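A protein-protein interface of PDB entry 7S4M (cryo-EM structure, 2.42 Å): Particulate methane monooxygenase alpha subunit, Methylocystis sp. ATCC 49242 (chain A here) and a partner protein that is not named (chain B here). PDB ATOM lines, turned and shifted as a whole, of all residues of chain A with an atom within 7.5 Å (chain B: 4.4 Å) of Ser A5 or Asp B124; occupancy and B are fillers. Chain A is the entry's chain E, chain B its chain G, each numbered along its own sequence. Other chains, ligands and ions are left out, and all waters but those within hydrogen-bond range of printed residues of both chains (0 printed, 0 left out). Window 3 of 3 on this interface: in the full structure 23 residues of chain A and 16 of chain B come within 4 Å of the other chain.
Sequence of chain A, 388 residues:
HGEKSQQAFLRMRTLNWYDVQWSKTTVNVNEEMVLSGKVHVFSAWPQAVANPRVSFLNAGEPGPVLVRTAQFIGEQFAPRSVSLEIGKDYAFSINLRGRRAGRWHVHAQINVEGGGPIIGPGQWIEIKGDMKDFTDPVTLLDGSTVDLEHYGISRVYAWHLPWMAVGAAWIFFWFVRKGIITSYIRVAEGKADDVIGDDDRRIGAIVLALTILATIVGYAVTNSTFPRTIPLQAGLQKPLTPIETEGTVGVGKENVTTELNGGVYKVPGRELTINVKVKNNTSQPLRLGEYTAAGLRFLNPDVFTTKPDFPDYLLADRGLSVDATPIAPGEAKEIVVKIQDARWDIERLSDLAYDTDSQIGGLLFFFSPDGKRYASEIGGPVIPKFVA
A ring nitrogen (ND1) of His A1 sits close to the side-chain carboxylate (OD1) of Asp B37, at 3.3 Å. The side-chain hydroxyl (OG) of Ser A5 sits at hydrogen-bond distance from the backbone carbonyl oxygen (O) of Asp B124, at 2.9 Å.
Among the printed residues, pairs that only touch across the chains: Gly A2 with Asp B124, Ile A119 with Ile B122, Arg A348 with Phe B39, Lys A4 with Phe B39, His A1 with Ile B122, Ser A5 with Phe B39 and His A1 with Asp B124.
Hydrophobic or aromatic side chains of chain B that line the printed part of chain A: Phe B39 and Ile B122. Of the 14 printed residues of chain A, 6 touch a printed residue of chain B. Hydrophobic or aromatic side chains of chain A within 4 Å of the printed part of chain B: His A1 and Ile A119. Among the printed residues, no Asp or Glu carboxylate lies within 4 Å of a Lys or Arg side-chain nitrogen of the other chain.
Of the printed residues of chain B, Lys A4 touches Phe B39. Ser A5 touches just these residues of chain B: Phe B39 and Asp B124. Of the printed residues of chain A, Ile B122 touches His A1 and Ile A119. Of chain A, only His A1, Gly A2 and Ser A5 come within 4 Å of Asp B124. The nearest printed residue of chain A that does not touch Asp B37 is Lys A4 (4.3 Å).
NH2 of Arg A11 lies within hydrogen-bond range of O of Arg A348 (3.1 Å). The guanidinium group (NE) of Arg A348 is in salt-bridge range of the side-chain carboxylate (OD2) of Asp A351, at 3.0 Å. N of Phe B39 is in hydrogen-bond range of OD2 of Asp B37 (3.1 Å). O of Lys A4 is in hydrogen-bond range of NH1 of Arg A348. The side-chain carboxylate (OE1) of Glu A3 sits close to the backbone NH (N) of His A1 (3.3 Å). The backbone NH (N) of Ser B38 sits at hydrogen-bond distance from the side-chain carboxylate (OD2) of Asp B124 (3.0 Å).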
ATOM      1  N   HIS A   1      -9.804 -27.956 -20.377  1.00  0.00           N
ATOM      2  CA  HIS A   1     -10.544 -27.114 -21.305  1.00  0.00           C
ATOM      3  C   HIS A   1     -12.037 -27.392 -21.210  1.00  0.00           C
ATOM      4  O   HIS A   1     -12.854 -26.645 -21.741  1.00  0.00           O
ATOM      5  CB  HIS A   1     -10.059 -27.331 -22.734  1.00  0.00           C
ATOM      6  CG  HIS A   1     -10.132 -26.106 -23.586  1.00  0.00           C
ATOM      7  ND1 HIS A   1     -11.003 -25.072 -23.326  1.00  0.00           N
ATOM      8  CD2 HIS A   1      -9.444 -25.748 -24.696  1.00  0.00           C
ATOM      9  CE1 HIS A   1     -10.848 -24.129 -24.238  1.00  0.00           C
ATOM     10  NE2 HIS A   1      -9.908 -24.515 -25.080  1.00  0.00           N
ATOM     11  N   GLY A   2     -12.384 -28.481 -20.530  1.00  0.00           N
ATOM     12  CA  GLY A   2     -13.771 -28.865 -20.374  1.00  0.00           C
ATOM     13  C   GLY A   2     -14.341 -28.545 -19.009  1.00  0.00           C
ATOM     14  O   GLY A   2     -15.376 -29.090 -18.621  1.00  0.00           O
ATOM     15  N   GLU A   3     -13.670 -27.662 -18.268  1.00  0.00           N
ATOM     16  CA  GLU A   3     -14.112 -27.337 -16.917  1.00  0.00           C
ATOM     17  C   GLU A   3     -15.462 -26.636 -16.899  1.00  0.00           C
ATOM     18  O   GLU A   3     -16.104 -26.586 -15.845  1.00  0.00           O
ATOM     19  CB  GLU A   3     -13.074 -26.462 -16.220  1.00  0.00           C
ATOM     20  CG  GLU A   3     -12.982 -25.054 -16.777  1.00  0.00           C
ATOM     21  CD  GLU A   3     -12.156 -24.980 -18.041  1.00  0.00           C
ATOM     22  OE1 GLU A   3     -11.557 -26.007 -18.419  1.00  0.00           O
ATOM     23  OE2 GLU A   3     -12.106 -23.897 -18.658  1.00  0.00           O
ATOM     24  N   LYS A   4     -15.903 -26.089 -18.032  1.00  0.00           N
ATOM     25  CA  LYS A   4     -17.191 -25.406 -18.062  1.00  0.00           C
ATOM     26  C   LYS A   4     -18.335 -26.365 -17.769  1.00  0.00           C
ATOM     27  O   LYS A   4     -19.306 -25.998 -17.099  1.00  0.00           O
ATOM     28  CB  LYS A   4     -17.396 -24.734 -19.418  1.00  0.00           C
ATOM     29  CG  LYS A   4     -17.421 -23.224 -19.358  1.00  0.00           C
ATOM     30  CD  LYS A   4     -16.710 -22.624 -20.552  1.00  0.00           C
ATOM     31  CE  LYS A   4     -17.668 -22.426 -21.709  1.00  0.00           C
ATOM     32  NZ  LYS A   4     -16.970 -21.912 -22.917  1.00  0.00           N
ATOM     33  N   SER A   5     -18.240 -27.596 -18.263  1.00  0.00           N
ATOM     34  CA  SER A   5     -19.308 -28.568 -18.082  1.00  0.00           C
ATOM     35  C   SER A   5     -19.372 -29.137 -16.673  1.00  0.00           C
ATOM     36  O   SER A   5     -20.407 -29.699 -16.300  1.00  0.00           O
ATOM     37  CB  SER A   5     -19.150 -29.708 -19.084  1.00  0.00           C
ATOM     38  OG  SER A   5     -17.984 -30.462 -18.809  1.00  0.00           O
ATOM     39  N   GLN A   6     -18.308 -29.017 -15.886  1.00  0.00           N
ATOM     40  CA  GLN A   6     -18.332 -29.540 -14.529  1.00  0.00           C
ATOM     41  C   GLN A   6     -19.284 -28.726 -13.662  1.00  0.00           C
ATOM     42  O   GLN A   6     -19.550 -27.551 -13.925  1.00  0.00           O
ATOM     43  CB  GLN A   6     -16.929 -29.529 -13.927  1.00  0.00           C
ATOM     44  CG  GLN A   6     -16.062 -30.683 -14.389  1.00  0.00           C
ATOM     45  CD  GLN A   6     -14.659 -30.618 -13.829  1.00  0.00           C
ATOM     46  OE1 GLN A   6     -14.189 -29.558 -13.422  1.00  0.00           O
ATOM     47  NE2 GLN A   6     -13.984 -31.758 -13.799  1.00  0.00           N
ATOM     48  N   GLN A   7     -19.805 -29.369 -12.619  1.00  0.00           N
ATOM     49  CA  GLN A   7     -20.783 -28.716 -11.761  1.00  0.00           C
ATOM     50  C   GLN A   7     -20.153 -27.545 -11.019  1.00  0.00           C
ATOM     51  O   GLN A   7     -19.000 -27.608 -10.584  1.00  0.00           O
ATOM     52  CB  GLN A   7     -21.378 -29.717 -10.774  1.00  0.00           C
ATOM     53  CG  GLN A   7     -22.451 -30.592 -11.390  1.00  0.00           C
ATOM     54  CD  GLN A   7     -23.236 -31.369 -10.361  1.00  0.00           C
ATOM     55  OE1 GLN A   7     -22.742 -32.338  -9.791  1.00  0.00           O
ATOM     56  NE2 GLN A   7     -24.471 -30.947 -10.117  1.00  0.00           N
ATOM     57  N   ALA A   8     -20.926 -26.468 -10.878  1.00  0.00           N
ATOM     58  CA  ALA A   8     -20.383 -25.225 -10.343  1.00  0.00           C
ATOM     59  C   ALA A   8     -19.978 -25.375  -8.883  1.00  0.00           C
ATOM     60  O   ALA A   8     -18.860 -25.010  -8.499  1.00  0.00           O
ATOM     61  CB  ALA A   8     -21.401 -24.099 -10.503  1.00  0.00           C
ATOM     62  N   ARG A  11     -16.883 -27.246  -8.433  1.00  0.00           N
ATOM     63  CA  ARG A  11     -15.716 -26.500  -8.887  1.00  0.00           C
ATOM     64  C   ARG A  11     -15.283 -25.470  -7.857  1.00  0.00           C
ATOM     65  O   ARG A  11     -14.084 -25.264  -7.639  1.00  0.00           O
ATOM     66  CB  ARG A  11     -16.012 -25.826 -10.224  1.00  0.00           C
ATOM     67  CG  ARG A  11     -15.590 -26.641 -11.426  1.00  0.00           C
ATOM     68  CD  ARG A  11     -15.836 -25.880 -12.711  1.00  0.00           C
ATOM     69  NE  ARG A  11     -17.241 -25.534 -12.881  1.00  0.00           N
ATOM     70  CZ  ARG A  11     -17.675 -24.524 -13.620  1.00  0.00           C
ATOM     71  NH1 ARG A  11     -16.837 -23.730 -14.265  1.00  0.00           N
ATOM     72  NH2 ARG A  11     -18.983 -24.302 -13.712  1.00  0.00           N
ATOM     73  N   ILE A 119      -9.954 -28.853 -12.613  1.00  0.00           N
ATOM     74  CA  ILE A 119      -9.231 -28.068 -13.605  1.00  0.00           C
ATOM     75  C   ILE A 119      -9.059 -26.652 -13.085  1.00  0.00           C
ATOM     76  O   ILE A 119     -10.034 -26.000 -12.696  1.00  0.00           O
ATOM     77  CB  ILE A 119      -9.964 -28.068 -14.955  1.00  0.00           C
ATOM     78  CG1 ILE A 119     -10.063 -29.490 -15.503  1.00  0.00           C
ATOM     79  CG2 ILE A 119      -9.251 -27.173 -15.944  1.00  0.00           C
ATOM     80  CD1 ILE A 119     -11.427 -30.108 -15.345  1.00  0.00           C
ATOM     81  N   GLU A 347     -18.365 -18.855 -17.801  1.00  0.00           N
ATOM     82  CA  GLU A 347     -17.706 -20.044 -17.194  1.00  0.00           C
ATOM     83  C   GLU A 347     -18.818 -20.929 -16.647  1.00  0.00           C
ATOM     84  O   GLU A 347     -18.488 -21.970 -16.042  1.00  0.00           O
ATOM     85  CB  GLU A 347     -16.674 -19.622 -16.150  1.00  0.00           C
ATOM     86  CG  GLU A 347     -15.401 -19.085 -16.774  1.00  0.00           C
ATOM     87  CD  GLU A 347     -14.875 -19.896 -17.946  1.00  0.00           C
ATOM     88  OE1 GLU A 347     -14.396 -21.025 -17.714  1.00  0.00           O
ATOM     89  OE2 GLU A 347     -14.941 -19.395 -19.086  1.00  0.00           O
ATOM     90  N   ARG A 348     -20.064 -20.478 -16.797  1.00  0.00           N
ATOM     91  CA  ARG A 348     -21.237 -21.310 -16.443  1.00  0.00           C
ATOM     92  C   ARG A 348     -21.273 -21.609 -14.941  1.00  0.00           C
ATOM     93  O   ARG A 348     -21.587 -22.757 -14.580  1.00  0.00           O
ATOM     94  CB  ARG A 348     -21.213 -22.502 -17.399  1.00  0.00           C
ATOM     95  CG  ARG A 348     -22.258 -22.438 -18.504  1.00  0.00           C
ATOM     96  CD  ARG A 348     -23.221 -23.607 -18.409  1.00  0.00           C
ATOM     97  NE  ARG A 348     -22.948 -24.324 -17.174  1.00  0.00           N
ATOM     98  CZ  ARG A 348     -22.251 -25.445 -17.088  1.00  0.00           C
ATOM     99  NH1 ARG A 348     -21.807 -26.030 -18.187  1.00  0.00           N
ATOM    100  NH2 ARG A 348     -22.026 -25.988 -15.904  1.00  0.00           N
ATOM    101  N   ASP A 351     -24.977 -21.680 -13.465  1.00  0.00           N
ATOM    102  CA  ASP A 351     -25.699 -22.943 -13.479  1.00  0.00           C
ATOM    103  C   ASP A 351     -25.743 -23.602 -12.114  1.00  0.00           C
ATOM    104  O   ASP A 351     -26.070 -24.791 -12.019  1.00  0.00           O
ATOM    105  CB  ASP A 351     -25.078 -23.896 -14.501  1.00  0.00           C
ATOM    106  CG  ASP A 351     -25.879 -23.976 -15.781  1.00  0.00           C
ATOM    107  OD1 ASP A 351     -26.631 -23.023 -16.070  1.00  0.00           O
ATOM    108  OD2 ASP A 351     -25.758 -24.990 -16.498  1.00  0.00           O
ATOM    109  N   ASP A 355     -27.467 -27.451  -9.908  1.00  0.00           N
ATOM    110  CA  ASP A 355     -26.772 -28.371  -9.024  1.00  0.00           C
ATOM    111  C   ASP A 355     -27.672 -28.807  -7.874  1.00  0.00           C
ATOM    112  O   ASP A 355     -28.671 -28.161  -7.548  1.00  0.00           O
ATOM    113  CB  ASP A 355     -25.500 -27.731  -8.477  1.00  0.00           C
ATOM    114  CG  ASP A 355     -24.460 -27.496  -9.549  1.00  0.00           C
ATOM    115  OD1 ASP A 355     -24.662 -27.972 -10.686  1.00  0.00           O
ATOM    116  OD2 ASP A 355     -23.441 -26.837  -9.260  1.00  0.00           O
ATOM    117  N   ASP B  37     -12.842 -28.013 -27.679  1.00  0.00           N
ATOM    118  CA  ASP B  37     -13.899 -27.409 -26.823  1.00  0.00           C
ATOM    119  C   ASP B  37     -15.277 -27.668 -27.429  1.00  0.00           C
ATOM    120  O   ASP B  37     -15.495 -27.247 -28.575  1.00  0.00           O
ATOM    121  CB  ASP B  37     -13.671 -25.916 -26.594  1.00  0.00           C
ATOM    122  CG  ASP B  37     -14.529 -25.374 -25.466  1.00  0.00           C
ATOM    123  OD1 ASP B  37     -14.155 -25.572 -24.297  1.00  0.00           O
ATOM    124  OD2 ASP B  37     -15.572 -24.771 -25.767  1.00  0.00           O
ATOM    125  N   SER B  38     -16.171 -28.293 -26.665  1.00  0.00           N
ATOM    126  CA  SER B  38     -17.509 -28.622 -27.132  1.00  0.00           C
ATOM    127  C   SER B  38     -18.501 -27.481 -26.971  1.00  0.00           C
ATOM    128  O   SER B  38     -19.619 -27.577 -27.485  1.00  0.00           O
ATOM    129  CB  SER B  38     -18.041 -29.851 -26.391  1.00  0.00           C
ATOM    130  OG  SER B  38     -18.282 -29.555 -25.029  1.00  0.00           O
ATOM    131  N   PHE B  39     -18.129 -26.411 -26.271  1.00  0.00           N
ATOM    132  CA  PHE B  39     -19.028 -25.279 -26.100  1.00  0.00           C
ATOM    133  C   PHE B  39     -18.807 -24.188 -27.134  1.00  0.00           C
ATOM    134  O   PHE B  39     -19.679 -23.327 -27.301  1.00  0.00           O
ATOM    135  CB  PHE B  39     -18.876 -24.690 -24.697  1.00  0.00           C
ATOM    136  CG  PHE B  39     -19.634 -25.441 -23.645  1.00  0.00           C
ATOM    137  CD1 PHE B  39     -19.050 -26.501 -22.979  1.00  0.00           C
ATOM    138  CD2 PHE B  39     -20.933 -25.090 -23.328  1.00  0.00           C
ATOM    139  CE1 PHE B  39     -19.746 -27.196 -22.012  1.00  0.00           C
ATOM    140  CE2 PHE B  39     -21.635 -25.781 -22.362  1.00  0.00           C
ATOM    141  CZ  PHE B  39     -21.040 -26.836 -21.702  1.00  0.00           C
ATOM    142  N   ILE B 122     -10.374 -33.663 -21.305  1.00  0.00           N
ATOM    143  CA  ILE B 122     -10.925 -33.944 -19.992  1.00  0.00           C
ATOM    144  C   ILE B 122     -12.426 -34.229 -20.076  1.00  0.00           C
ATOM    145  O   ILE B 122     -13.156 -34.023 -19.108  1.00  0.00           O
ATOM    146  CB  ILE B 122     -10.614 -32.808 -19.007  1.00  0.00           C
ATOM    147  CG1 ILE B 122      -9.205 -32.285 -19.264  1.00  0.00           C
ATOM    148  CG2 ILE B 122     -10.662 -33.311 -17.578  1.00  0.00           C
ATOM    149  CD1 ILE B 122      -8.813 -31.121 -18.394  1.00  0.00           C
ATOM    150  N   ARG B 123     -12.897 -34.692 -21.236  1.00  0.00           N
ATOM    151  CA  ARG B 123     -14.288 -35.081 -21.455  1.00  0.00           C
ATOM    152  C   ARG B 123     -15.236 -33.904 -21.207  1.00  0.00           C
ATOM    153  O   ARG B 123     -16.019 -33.877 -20.259  1.00  0.00           O
ATOM    154  CB  ARG B 123     -14.660 -36.289 -20.588  1.00  0.00           C
ATOM    155  CG  ARG B 123     -13.790 -37.501 -20.839  1.00  0.00           C
ATOM    156  CD  ARG B 123     -14.633 -38.751 -20.912  1.00  0.00           C
ATOM    157  NE  ARG B 123     -15.714 -38.595 -21.877  1.00  0.00           N
ATOM    158  CZ  ARG B 123     -16.997 -38.520 -21.554  1.00  0.00           C
ATOM    159  NH1 ARG B 123     -17.399 -38.606 -20.297  1.00  0.00           N
ATOM    160  NH2 ARG B 123     -17.898 -38.350 -22.516  1.00  0.00           N
ATOM    161  N   ASP B 124     -15.114 -32.909 -22.091  1.00  0.00           N
ATOM    162  CA  ASP B 124     -15.995 -31.748 -22.029  1.00  0.00           C
ATOM    163  C   ASP B 124     -17.465 -32.146 -22.087  1.00  0.00           C
ATOM    164  O   ASP B 124     -18.309 -31.492 -21.465  1.00  0.00           O
ATOM    165  CB  ASP B 124     -15.664 -30.781 -23.167  1.00  0.00           C
ATOM    166  CG  ASP B 124     -16.110 -29.361 -22.878  1.00  0.00           C
ATOM    167  OD1 ASP B 124     -16.795 -29.143 -21.857  1.00  0.00           O
ATOM    168  OD2 ASP B 124     -15.777 -28.460 -23.677  1.00  0.00           O
ATOM    169  N   THR B 125     -17.794 -33.209 -22.817  1.00  0.00           N
ATOM    170  CA  THR B 125     -19.172 -33.662 -22.931  1.00  0.00           C
ATOM    171  C   THR B 125     -19.181 -35.130 -23.332  1.00  0.00           C
ATOM    172  O   THR B 125     -18.132 -35.754 -23.515  1.00  0.00           O
ATOM    173  CB  THR B 125     -19.953 -32.820 -23.944  1.00  0.00           C
ATOM    174  OG1 THR B 125     -21.331 -33.215 -23.932  1.00  0.00           O
ATOM    175  CG2 THR B 125     -19.391 -33.021 -25.342  1.00  0.00           C
